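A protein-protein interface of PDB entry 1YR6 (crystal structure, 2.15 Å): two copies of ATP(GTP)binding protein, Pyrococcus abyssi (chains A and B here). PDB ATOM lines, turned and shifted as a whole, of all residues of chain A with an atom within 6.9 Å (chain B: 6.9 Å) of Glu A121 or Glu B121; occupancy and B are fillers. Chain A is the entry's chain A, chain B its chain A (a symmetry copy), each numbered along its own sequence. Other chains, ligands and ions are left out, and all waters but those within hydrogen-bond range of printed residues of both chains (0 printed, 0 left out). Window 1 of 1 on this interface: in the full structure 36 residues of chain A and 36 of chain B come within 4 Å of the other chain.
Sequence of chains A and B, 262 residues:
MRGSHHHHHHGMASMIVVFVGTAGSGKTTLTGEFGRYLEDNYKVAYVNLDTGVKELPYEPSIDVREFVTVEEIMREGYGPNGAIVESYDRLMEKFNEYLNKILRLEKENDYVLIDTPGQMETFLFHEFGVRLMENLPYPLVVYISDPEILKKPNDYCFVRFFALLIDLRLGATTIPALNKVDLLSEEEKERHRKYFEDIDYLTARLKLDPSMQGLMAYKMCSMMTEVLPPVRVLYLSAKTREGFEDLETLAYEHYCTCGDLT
The side-chain carboxylate (OE1) of Glu A121 sits at hydrogen-bond distance from the backbone NH (N) of Met B120, 3.2 Å away. The side-chain carboxylate (OE2) of Glu B121 sits close to the side-chain carboxylate (OE2) of Glu A121 (2.7 Å). OE2 of Glu A121 sits close to OE1 of Gln B119 (2.7 Å). The side-chain carboxylate (OE2) of Glu B121 lies close to the side-chain amide oxygen (OE1) of Gln A119 (2.7 Å). OE1 of Glu B121 is in hydrogen-bond range of N of Met A120 (3.2 Å).
N of Ala A23 sits at hydrogen-bond distance from O of Gly A118, 2.7 Å away. O of Gly B118 sits at hydrogen-bond distance from N of Ala B23, 2.7 Å away. The side-chain hydroxyl (OG1) of Thr A122 lies close to the backbone carbonyl oxygen (O) of Gln A119 (3.3 Å). The side-chain hydroxyl of Thr B122 lies close to the backbone carbonyl oxygen of Gln B119 (3.3 Å).
CG2 of Thr A22 touches OE1 of Glu B121 (3.2 Å). Thr A22 touches Phe B125 (CG2 to CD2, 3.9 Å). Gly A118 touches Glu B121 (O to OE1, 3.7 Å). Gln A119 touches Gln B119 (OE1 to OE1, 3.5 Å). CG2 of Thr B22 touches OE1 of Glu A121 (3.2 Å). OE1 of Glu A121 touches O of Gly B118, at 3.7 Å. CD2 of Phe A125 touches CG2 of Thr B22 (3.9 Å). Phe B162 touches Phe A162 (CE1 to CE1, 3.8 Å).
Of the printed residues of chain B, Met A120 touches Glu B121. Glu A121 touches just these residues of chain B: Thr B22 (3.2 Å), Gly B118 (3.7 Å), Gln B119 (2.7 Å), Met B120 (3.2 Å) and Glu B121 (2.7 Å). Of the printed residues of chain A, Thr B22 touches Glu A121 and Phe A125. Printed residues of chain A within 4 Å of Gln B119: Gln A119 and Glu A121. Of the printed residues of chain A, Met B120 touches Glu A121. Glu B121 touches just these residues of chain A: Thr A22, Gly A118, Gln A119, Met A120 and Glu A121. Of the printed residues of chain A, Phe B125 touches Thr A22. The nearest printed residue of chain B that does not touch Phe A162 is Phe B125 (4.2 Å).
Hydrophobic or aromatic side chains of chain A that line the printed part of chain B: Met A120, Phe A125 and Phe A162. Of the 14 printed residues of chain B, 7 touch a printed residue of chain A. Hydrophobic or aromatic side chains of chain B within 4 Å of the printed part of chain A: Met B120, Phe B125 and Phe B162. Along chain B the printed residues that touch a printed residue of chain A span positions 22 to 162.
Thr A22 touches Phe B125, and with the chains exchanged Phe A125 touches Thr B22. Gln A119 touches its own counterpart, Gln B119. Met A120 touches Glu B121, and with the chains exchanged Glu A121 touches Met B120. Glu B121 touches its own counterpart, Glu A121. 14 positions are printed for both chains. Of the 13 pairs that touch across the chains among the printed residues, 13 have their exchanged pair printed and touching as well.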
ATOM      1  N   GLY A  21       7.076  18.752 -24.033  1.00  0.00           N
ATOM      2  CA  GLY A  21       7.931  18.224 -22.988  1.00  0.00           C
ATOM      3  C   GLY A  21       7.869  16.717 -23.006  1.00  0.00           C
ATOM      4  O   GLY A  21       6.855  16.148 -23.456  1.00  0.00           O
ATOM      5  N   THR A  22       8.927  16.065 -22.511  1.00  0.00           N
ATOM      6  CA  THR A  22       8.994  14.590 -22.480  1.00  0.00           C
ATOM      7  C   THR A  22       8.202  14.035 -21.319  1.00  0.00           C
ATOM      8  O   THR A  22       8.093  14.670 -20.264  1.00  0.00           O
ATOM      9  CB  THR A  22      10.450  14.026 -22.321  1.00  0.00           C
ATOM     10  OG1 THR A  22      10.982  14.393 -21.038  1.00  0.00           O
ATOM     11  CG2 THR A  22      11.357  14.533 -23.386  1.00  0.00           C
ATOM     12  N   ALA A  23       7.690  12.820 -21.511  1.00  0.00           N
ATOM     13  CA  ALA A  23       6.893  12.130 -20.500  1.00  0.00           C
ATOM     14  C   ALA A  23       7.672  12.011 -19.190  1.00  0.00           C
ATOM     15  O   ALA A  23       8.737  11.395 -19.156  1.00  0.00           O
ATOM     16  CB  ALA A  23       6.480  10.747 -21.011  1.00  0.00           C
ATOM     17  N   PRO A 117       1.773  15.140 -27.292  1.00  0.00           N
ATOM     18  CA  PRO A 117       2.165  13.784 -26.920  1.00  0.00           C
ATOM     19  C   PRO A 117       3.337  13.707 -25.946  1.00  0.00           C
ATOM     20  O   PRO A 117       4.377  14.324 -26.152  1.00  0.00           O
ATOM     21  CB  PRO A 117       2.555  13.171 -28.251  1.00  0.00           C
ATOM     22  CG  PRO A 117       1.724  13.876 -29.245  1.00  0.00           C
ATOM     23  CD  PRO A 117       1.672  15.300 -28.753  1.00  0.00           C
ATOM     24  N   GLY A 118       3.153  12.945 -24.882  1.00  0.00           N
ATOM     25  CA  GLY A 118       4.211  12.677 -23.925  1.00  0.00           C
ATOM     26  C   GLY A 118       5.486  12.189 -24.558  1.00  0.00           C
ATOM     27  O   GLY A 118       6.537  12.242 -23.926  1.00  0.00           O
ATOM     28  N   GLN A 119       5.411  11.707 -25.798  1.00  0.00           N
ATOM     29  CA  GLN A 119       6.623  11.368 -26.564  1.00  0.00           C
ATOM     30  C   GLN A 119       6.879  12.472 -27.582  1.00  0.00           C
ATOM     31  O   GLN A 119       6.396  12.415 -28.705  1.00  0.00           O
ATOM     32  CB  GLN A 119       6.483  10.004 -27.264  1.00  0.00           C
ATOM     33  CG  GLN A 119       6.160   8.828 -26.333  1.00  0.00           C
ATOM     34  CD  GLN A 119       7.294   8.519 -25.368  1.00  0.00           C
ATOM     35  OE1 GLN A 119       8.460   8.799 -25.655  1.00  0.00           O
ATOM     36  NE2 GLN A 119       6.956   7.970 -24.210  1.00  0.00           N
ATOM     37  N   MET A 120       7.639  13.483 -27.186  1.00  0.00           N
ATOM     38  CA  MET A 120       7.706  14.712 -27.987  1.00  0.00           C
ATOM     39  C   MET A 120       8.198  14.539 -29.431  1.00  0.00           C
ATOM     40  O   MET A 120       7.925  15.384 -30.290  1.00  0.00           O
ATOM     41  CB  MET A 120       8.463  15.829 -27.262  1.00  0.00           C
ATOM     42  CG  MET A 120       9.810  15.464 -26.741  1.00  0.00           C
ATOM     43  SD  MET A 120      10.572  16.852 -25.854  1.00  0.00           S
ATOM     44  CE  MET A 120      10.319  18.126 -27.067  1.00  0.00           C
ATOM     45  N   GLU A 121       8.884  13.439 -29.713  1.00  0.00           N
ATOM     46  CA  GLU A 121       9.288  13.161 -31.082  1.00  0.00           C
ATOM     47  C   GLU A 121       8.098  12.734 -31.938  1.00  0.00           C
ATOM     48  O   GLU A 121       8.094  12.934 -33.154  1.00  0.00           O
ATOM     49  CB  GLU A 121      10.330  12.064 -31.096  1.00  0.00           C
ATOM     50  CG  GLU A 121       9.705  10.693 -30.982  1.00  0.00           C
ATOM     51  CD  GLU A 121      10.633   9.717 -30.348  1.00  0.00           C
ATOM     52  OE1 GLU A 121      11.507   9.178 -31.063  1.00  0.00           O
ATOM     53  OE2 GLU A 121      10.484   9.506 -29.125  1.00  0.00           O
ATOM     54  N   THR A 122       7.102  12.122 -31.299  1.00  0.00           N
ATOM     55  CA  THR A 122       5.800  11.906 -31.913  1.00  0.00           C
ATOM     56  C   THR A 122       5.132  13.219 -32.258  1.00  0.00           C
ATOM     57  O   THR A 122       4.157  13.248 -33.010  1.00  0.00           O
ATOM     58  CB  THR A 122       4.864  11.186 -30.944  1.00  0.00           C
ATOM     59  OG1 THR A 122       5.414   9.896 -30.623  1.00  0.00           O
ATOM     60  CG2 THR A 122       3.517  11.031 -31.553  1.00  0.00           C
ATOM     61  N   PHE A 123       5.625  14.308 -31.680  1.00  0.00           N
ATOM     62  CA  PHE A 123       5.167  15.633 -32.080  1.00  0.00           C
ATOM     63  C   PHE A 123       6.177  16.293 -33.014  1.00  0.00           C
ATOM     64  O   PHE A 123       5.810  16.988 -33.933  1.00  0.00           O
ATOM     65  CB  PHE A 123       4.885  16.521 -30.863  1.00  0.00           C
ATOM     66  CG  PHE A 123       4.013  17.704 -31.174  1.00  0.00           C
ATOM     67  CD1 PHE A 123       2.687  17.523 -31.532  1.00  0.00           C
ATOM     68  CD2 PHE A 123       4.525  18.992 -31.139  1.00  0.00           C
ATOM     69  CE1 PHE A 123       1.881  18.602 -31.835  1.00  0.00           C
ATOM     70  CE2 PHE A 123       3.718  20.080 -31.424  1.00  0.00           C
ATOM     71  CZ  PHE A 123       2.396  19.887 -31.779  1.00  0.00           C
ATOM     72  N   LEU A 124       7.457  16.043 -32.788  1.00  0.00           N
ATOM     73  CA  LEU A 124       8.502  16.690 -33.566  1.00  0.00           C
ATOM     74  C   LEU A 124       8.687  16.073 -34.943  1.00  0.00           C
ATOM     75  O   LEU A 124       9.041  16.761 -35.910  1.00  0.00           O
ATOM     76  CB  LEU A 124       9.824  16.647 -32.812  1.00  0.00           C
ATOM     77  CG  LEU A 124       9.975  17.793 -31.831  1.00  0.00           C
ATOM     78  CD1 LEU A 124      11.310  17.704 -31.134  1.00  0.00           C
ATOM     79  CD2 LEU A 124       9.824  19.136 -32.571  1.00  0.00           C
ATOM     80  N   PHE A 125       8.454  14.779 -35.044  1.00  0.00           N
ATOM     81  CA  PHE A 125       8.755  14.116 -36.288  1.00  0.00           C
ATOM     82  C   PHE A 125       7.512  13.793 -37.125  1.00  0.00           C
ATOM     83  O   PHE A 125       7.429  14.141 -38.306  1.00  0.00           O
ATOM     84  CB  PHE A 125       9.687  12.920 -36.016  1.00  0.00           C
ATOM     85  CG  PHE A 125      11.022  13.343 -35.463  1.00  0.00           C
ATOM     86  CD1 PHE A 125      12.105  13.524 -36.303  1.00  0.00           C
ATOM     87  CD2 PHE A 125      11.177  13.624 -34.122  1.00  0.00           C
ATOM     88  CE1 PHE A 125      13.345  13.942 -35.808  1.00  0.00           C
ATOM     89  CE2 PHE A 125      12.411  14.041 -33.613  1.00  0.00           C
ATOM     90  CZ  PHE A 125      13.499  14.194 -34.469  1.00  0.00           C
ATOM     91  N   HIS A 126       6.512  13.193 -36.509  1.00  0.00           N
ATOM     92  CA  HIS A 126       5.358  12.720 -37.264  1.00  0.00           C
ATOM     93  C   HIS A 126       4.588  13.873 -37.920  1.00  0.00           C
ATOM     94  O   HIS A 126       4.505  14.943 -37.354  1.00  0.00           O
ATOM     95  CB  HIS A 126       4.442  11.913 -36.343  1.00  0.00           C
ATOM     96  CG  HIS A 126       3.281  11.279 -37.046  1.00  0.00           C
ATOM     97  ND1 HIS A 126       2.207  12.006 -37.508  1.00  0.00           N
ATOM     98  CD2 HIS A 126       3.026   9.986 -37.361  1.00  0.00           C
ATOM     99  CE1 HIS A 126       1.335  11.190 -38.074  1.00  0.00           C
ATOM    100  NE2 HIS A 126       1.810   9.960 -38.000  1.00  0.00           N
ATOM    101  N   PHE A 162      17.864  22.548 -27.667  1.00  0.00           N
ATOM    102  CA  PHE A 162      16.687  21.763 -28.049  1.00  0.00           C
ATOM    103  C   PHE A 162      15.489  22.666 -28.303  1.00  0.00           C
ATOM    104  O   PHE A 162      14.819  22.542 -29.324  1.00  0.00           O
ATOM    105  CB  PHE A 162      16.353  20.692 -27.008  1.00  0.00           C
ATOM    106  CG  PHE A 162      15.371  19.694 -27.502  1.00  0.00           C
ATOM    107  CD1 PHE A 162      15.729  18.790 -28.488  1.00  0.00           C
ATOM    108  CD2 PHE A 162      14.070  19.699 -27.048  1.00  0.00           C
ATOM    109  CE1 PHE A 162      14.808  17.877 -28.976  1.00  0.00           C
ATOM    110  CE2 PHE A 162      13.148  18.793 -27.537  1.00  0.00           C
ATOM    111  CZ  PHE A 162      13.515  17.890 -28.502  1.00  0.00           C
ATOM    112  N   GLY B  21      17.619   6.732 -33.739  1.00  0.00           N
ATOM    113  CA  GLY B  21      16.594   7.054 -34.713  1.00  0.00           C
ATOM    114  C   GLY B  21      15.235   6.832 -34.098  1.00  0.00           C
ATOM    115  O   GLY B  21      15.106   6.012 -33.170  1.00  0.00           O
ATOM    116  N   THR B  22      14.220   7.537 -34.612  1.00  0.00           N
ATOM    117  CA  THR B  22      12.843   7.418 -34.093  1.00  0.00           C
ATOM    118  C   THR B  22      12.162   6.183 -34.636  1.00  0.00           C
ATOM    119  O   THR B  22      12.438   5.750 -35.761  1.00  0.00           O
ATOM    120  CB  THR B  22      11.917   8.627 -34.474  1.00  0.00           C
ATOM    121  OG1 THR B  22      11.717   8.663 -35.897  1.00  0.00           O
ATOM    122  CG2 THR B  22      12.494   9.925 -34.032  1.00  0.00           C
ATOM    123  N   ALA B  23      11.237   5.650 -33.841  1.00  0.00           N
ATOM    124  CA  ALA B  23      10.480   4.452 -34.201  1.00  0.00           C
ATOM    125  C   ALA B  23       9.766   4.649 -35.538  1.00  0.00           C
ATOM    126  O   ALA B  23       8.928   5.542 -35.667  1.00  0.00           O
ATOM    127  CB  ALA B  23       9.478   4.113 -33.096  1.00  0.00           C
ATOM    128  N   PRO B 117      16.647   2.715 -27.848  1.00  0.00           N
ATOM    129  CA  PRO B 117      15.191   2.776 -27.773  1.00  0.00           C
ATOM    130  C   PRO B 117      14.524   3.467 -28.959  1.00  0.00           C
ATOM    131  O   PRO B 117      14.897   4.569 -29.346  1.00  0.00           O
ATOM    132  CB  PRO B 117      14.954   3.575 -26.507  1.00  0.00           C
ATOM    133  CG  PRO B 117      16.120   3.276 -25.652  1.00  0.00           C
ATOM    134  CD  PRO B 117      17.280   3.201 -26.610  1.00  0.00           C
ATOM    135  N   GLY B 118      13.535   2.803 -29.531  1.00  0.00           N
ATOM    136  CA  GLY B 118      12.726   3.375 -30.593  1.00  0.00           C
ATOM    137  C   GLY B 118      12.164   4.729 -30.259  1.00  0.00           C
ATOM    138  O   GLY B 118      11.755   5.455 -31.160  1.00  0.00           O
ATOM    139  N   GLN B 119      12.133   5.082 -28.974  1.00  0.00           N
ATOM    140  CA  GLN B 119      11.766   6.449 -28.563  1.00  0.00           C
ATOM    141  C   GLN B 119      13.036   7.199 -28.185  1.00  0.00           C
ATOM    142  O   GLN B 119      13.459   7.182 -27.036  1.00  0.00           O
ATOM    143  CB  GLN B 119      10.773   6.434 -27.388  1.00  0.00           C
ATOM    144  CG  GLN B 119       9.480   5.646 -27.641  1.00  0.00           C
ATOM    145  CD  GLN B 119       8.613   6.279 -28.717  1.00  0.00           C
ATOM    146  OE1 GLN B 119       8.673   7.489 -28.945  1.00  0.00           O
ATOM    147  NE2 GLN B 119       7.826   5.462 -29.405  1.00  0.00           N
ATOM    148  N   MET B 120      13.650   7.859 -29.157  1.00  0.00           N
ATOM    149  CA  MET B 120      15.012   8.368 -28.956  1.00  0.00           C
ATOM    150  C   MET B 120      15.189   9.354 -27.792  1.00  0.00           C
ATOM    151  O   MET B 120      16.302   9.531 -27.286  1.00  0.00           O
ATOM    152  CB  MET B 120      15.621   8.910 -30.253  1.00  0.00           C
ATOM    153  CG  MET B 120      14.789   9.903 -30.991  1.00  0.00           C
ATOM    154  SD  MET B 120      15.593  10.419 -32.534  1.00  0.00           S
ATOM    155  CE  MET B 120      17.205  10.798 -31.892  1.00  0.00           C
ATOM    156  N   GLU B 121      14.101   9.966 -27.342  1.00  0.00           N
ATOM    157  CA  GLU B 121      14.180  10.830 -26.175  1.00  0.00           C
ATOM    158  C   GLU B 121      14.353  10.021 -24.892  1.00  0.00           C
ATOM    159  O   GLU B 121      14.921  10.507 -23.913  1.00  0.00           O
ATOM    160  CB  GLU B 121      12.922  11.666 -26.071  1.00  0.00           C
ATOM    161  CG  GLU B 121      11.785  10.893 -25.446  1.00  0.00           C
ATOM    162  CD  GLU B 121      10.462  11.388 -25.913  1.00  0.00           C
ATOM    163  OE1 GLU B 121       9.978  12.403 -25.362  1.00  0.00           O
ATOM    164  OE2 GLU B 121       9.918  10.758 -26.846  1.00  0.00           O
ATOM    165  N   THR B 122      13.836   8.793 -24.897  1.00  0.00           N
ATOM    166  CA  THR B 122      14.152   7.810 -23.870  1.00  0.00           C
ATOM    167  C   THR B 122      15.630   7.481 -23.863  1.00  0.00           C
ATOM    168  O   THR B 122      16.133   6.881 -22.914  1.00  0.00           O
ATOM    169  CB  THR B 122      13.417   6.500 -24.138  1.00  0.00           C
ATOM    170  OG1 THR B 122      11.998   6.733 -24.095  1.00  0.00           O
ATOM    171  CG2 THR B 122      13.800   5.482 -23.124  1.00  0.00           C
ATOM    172  N   PHE B 123      16.322   7.835 -24.939  1.00  0.00           N
ATOM    173  CA  PHE B 123      17.775   7.720 -24.957  1.00  0.00           C
ATOM    174  C   PHE B 123      18.427   9.080 -24.719  1.00  0.00           C
ATOM    175  O   PHE B 123      19.444   9.176 -24.074  1.00  0.00           O
ATOM    176  CB  PHE B 123      18.274   7.096 -26.265  1.00  0.00           C
ATOM    177  CG  PHE B 123      19.672   6.551 -26.174  1.00  0.00           C
ATOM    178  CD1 PHE B 123      19.946   5.453 -25.374  1.00  0.00           C
ATOM    179  CD2 PHE B 123      20.714   7.153 -26.861  1.00  0.00           C
ATOM    180  CE1 PHE B 123      21.228   4.953 -25.271  1.00  0.00           C
ATOM    181  CE2 PHE B 123      21.999   6.647 -26.777  1.00  0.00           C
ATOM    182  CZ  PHE B 123      22.261   5.550 -25.977  1.00  0.00           C
ATOM    183  N   LEU B 124      17.811  10.136 -25.224  1.00  0.00           N
ATOM    184  CA  LEU B 124      18.391  11.467 -25.128  1.00  0.00           C
ATOM    185  C   LEU B 124      18.217  12.096 -23.755  1.00  0.00           C
ATOM    186  O   LEU B 124      19.065  12.870 -23.292  1.00  0.00           O
ATOM    187  CB  LEU B 124      17.789  12.383 -26.184  1.00  0.00           C
ATOM    188  CG  LEU B 124      18.491  12.275 -27.523  1.00  0.00           C
ATOM    189  CD1 LEU B 124      17.860  13.221 -28.515  1.00  0.00           C
ATOM    190  CD2 LEU B 124      19.992  12.575 -27.349  1.00  0.00           C
ATOM    191  N   PHE B 125      17.121  11.774 -23.097  1.00  0.00           N
ATOM    192  CA  PHE B 125      16.831  12.451 -21.858  1.00  0.00           C
ATOM    193  C   PHE B 125      17.107  11.597 -20.615  1.00  0.00           C
ATOM    194  O   PHE B 125      17.818  12.015 -19.698  1.00  0.00           O
ATOM    195  CB  PHE B 125      15.420  13.064 -21.929  1.00  0.00           C
ATOM    196  CG  PHE B 125      15.303  14.123 -22.993  1.00  0.00           C
ATOM    197  CD1 PHE B 125      15.467  15.459 -22.677  1.00  0.00           C
ATOM    198  CD2 PHE B 125      15.099  13.782 -24.313  1.00  0.00           C
ATOM    199  CE1 PHE B 125      15.388  16.453 -23.658  1.00  0.00           C
ATOM    200  CE2 PHE B 125      15.016  14.765 -25.305  1.00  0.00           C
ATOM    201  CZ  PHE B 125      15.159  16.108 -24.965  1.00  0.00           C
ATOM    202  N   HIS B 126      16.609  10.376 -20.603  1.00  0.00           N
ATOM    203  CA  HIS B 126      16.699   9.555 -19.401  1.00  0.00           C
ATOM    204  C   HIS B 126      18.151   9.233 -19.032  1.00  0.00           C
ATOM    205  O   HIS B 126      18.974   9.061 -19.907  1.00  0.00           O
ATOM    206  CB  HIS B 126      15.894   8.270 -19.600  1.00  0.00           C
ATOM    207  CG  HIS B 126      15.822   7.404 -18.380  1.00  0.00           C
ATOM    208  ND1 HIS B 126      16.898   6.681 -17.919  1.00  0.00           N
ATOM    209  CD2 HIS B 126      14.799   7.145 -17.530  1.00  0.00           C
ATOM    210  CE1 HIS B 126      16.544   6.007 -16.840  1.00  0.00           C
ATOM    211  NE2 HIS B 126      15.276   6.272 -16.581  1.00  0.00           N
ATOM    212  N   PHE B 162      19.587  18.444 -35.455  1.00  0.00           N
ATOM    213  CA  PHE B 162      19.278  17.424 -34.450  1.00  0.00           C
ATOM    214  C   PHE B 162      20.481  16.527 -34.198  1.00  0.00           C
ATOM    215  O   PHE B 162      20.855  16.291 -33.053  1.00  0.00           O
ATOM    216  CB  PHE B 162      18.051  16.595 -34.836  1.00  0.00           C
ATOM    217  CG  PHE B 162      17.534  15.772 -33.714  1.00  0.00           C
ATOM    218  CD1 PHE B 162      16.930  16.376 -32.624  1.00  0.00           C
ATOM    219  CD2 PHE B 162      17.716  14.406 -33.698  1.00  0.00           C
ATOM    220  CE1 PHE B 162      16.474  15.616 -31.559  1.00  0.00           C
ATOM    221  CE2 PHE B 162      17.268  13.646 -32.634  1.00  0.00           C
ATOM    222  CZ  PHE B 162      16.655  14.251 -31.567  1.00  0.00           C
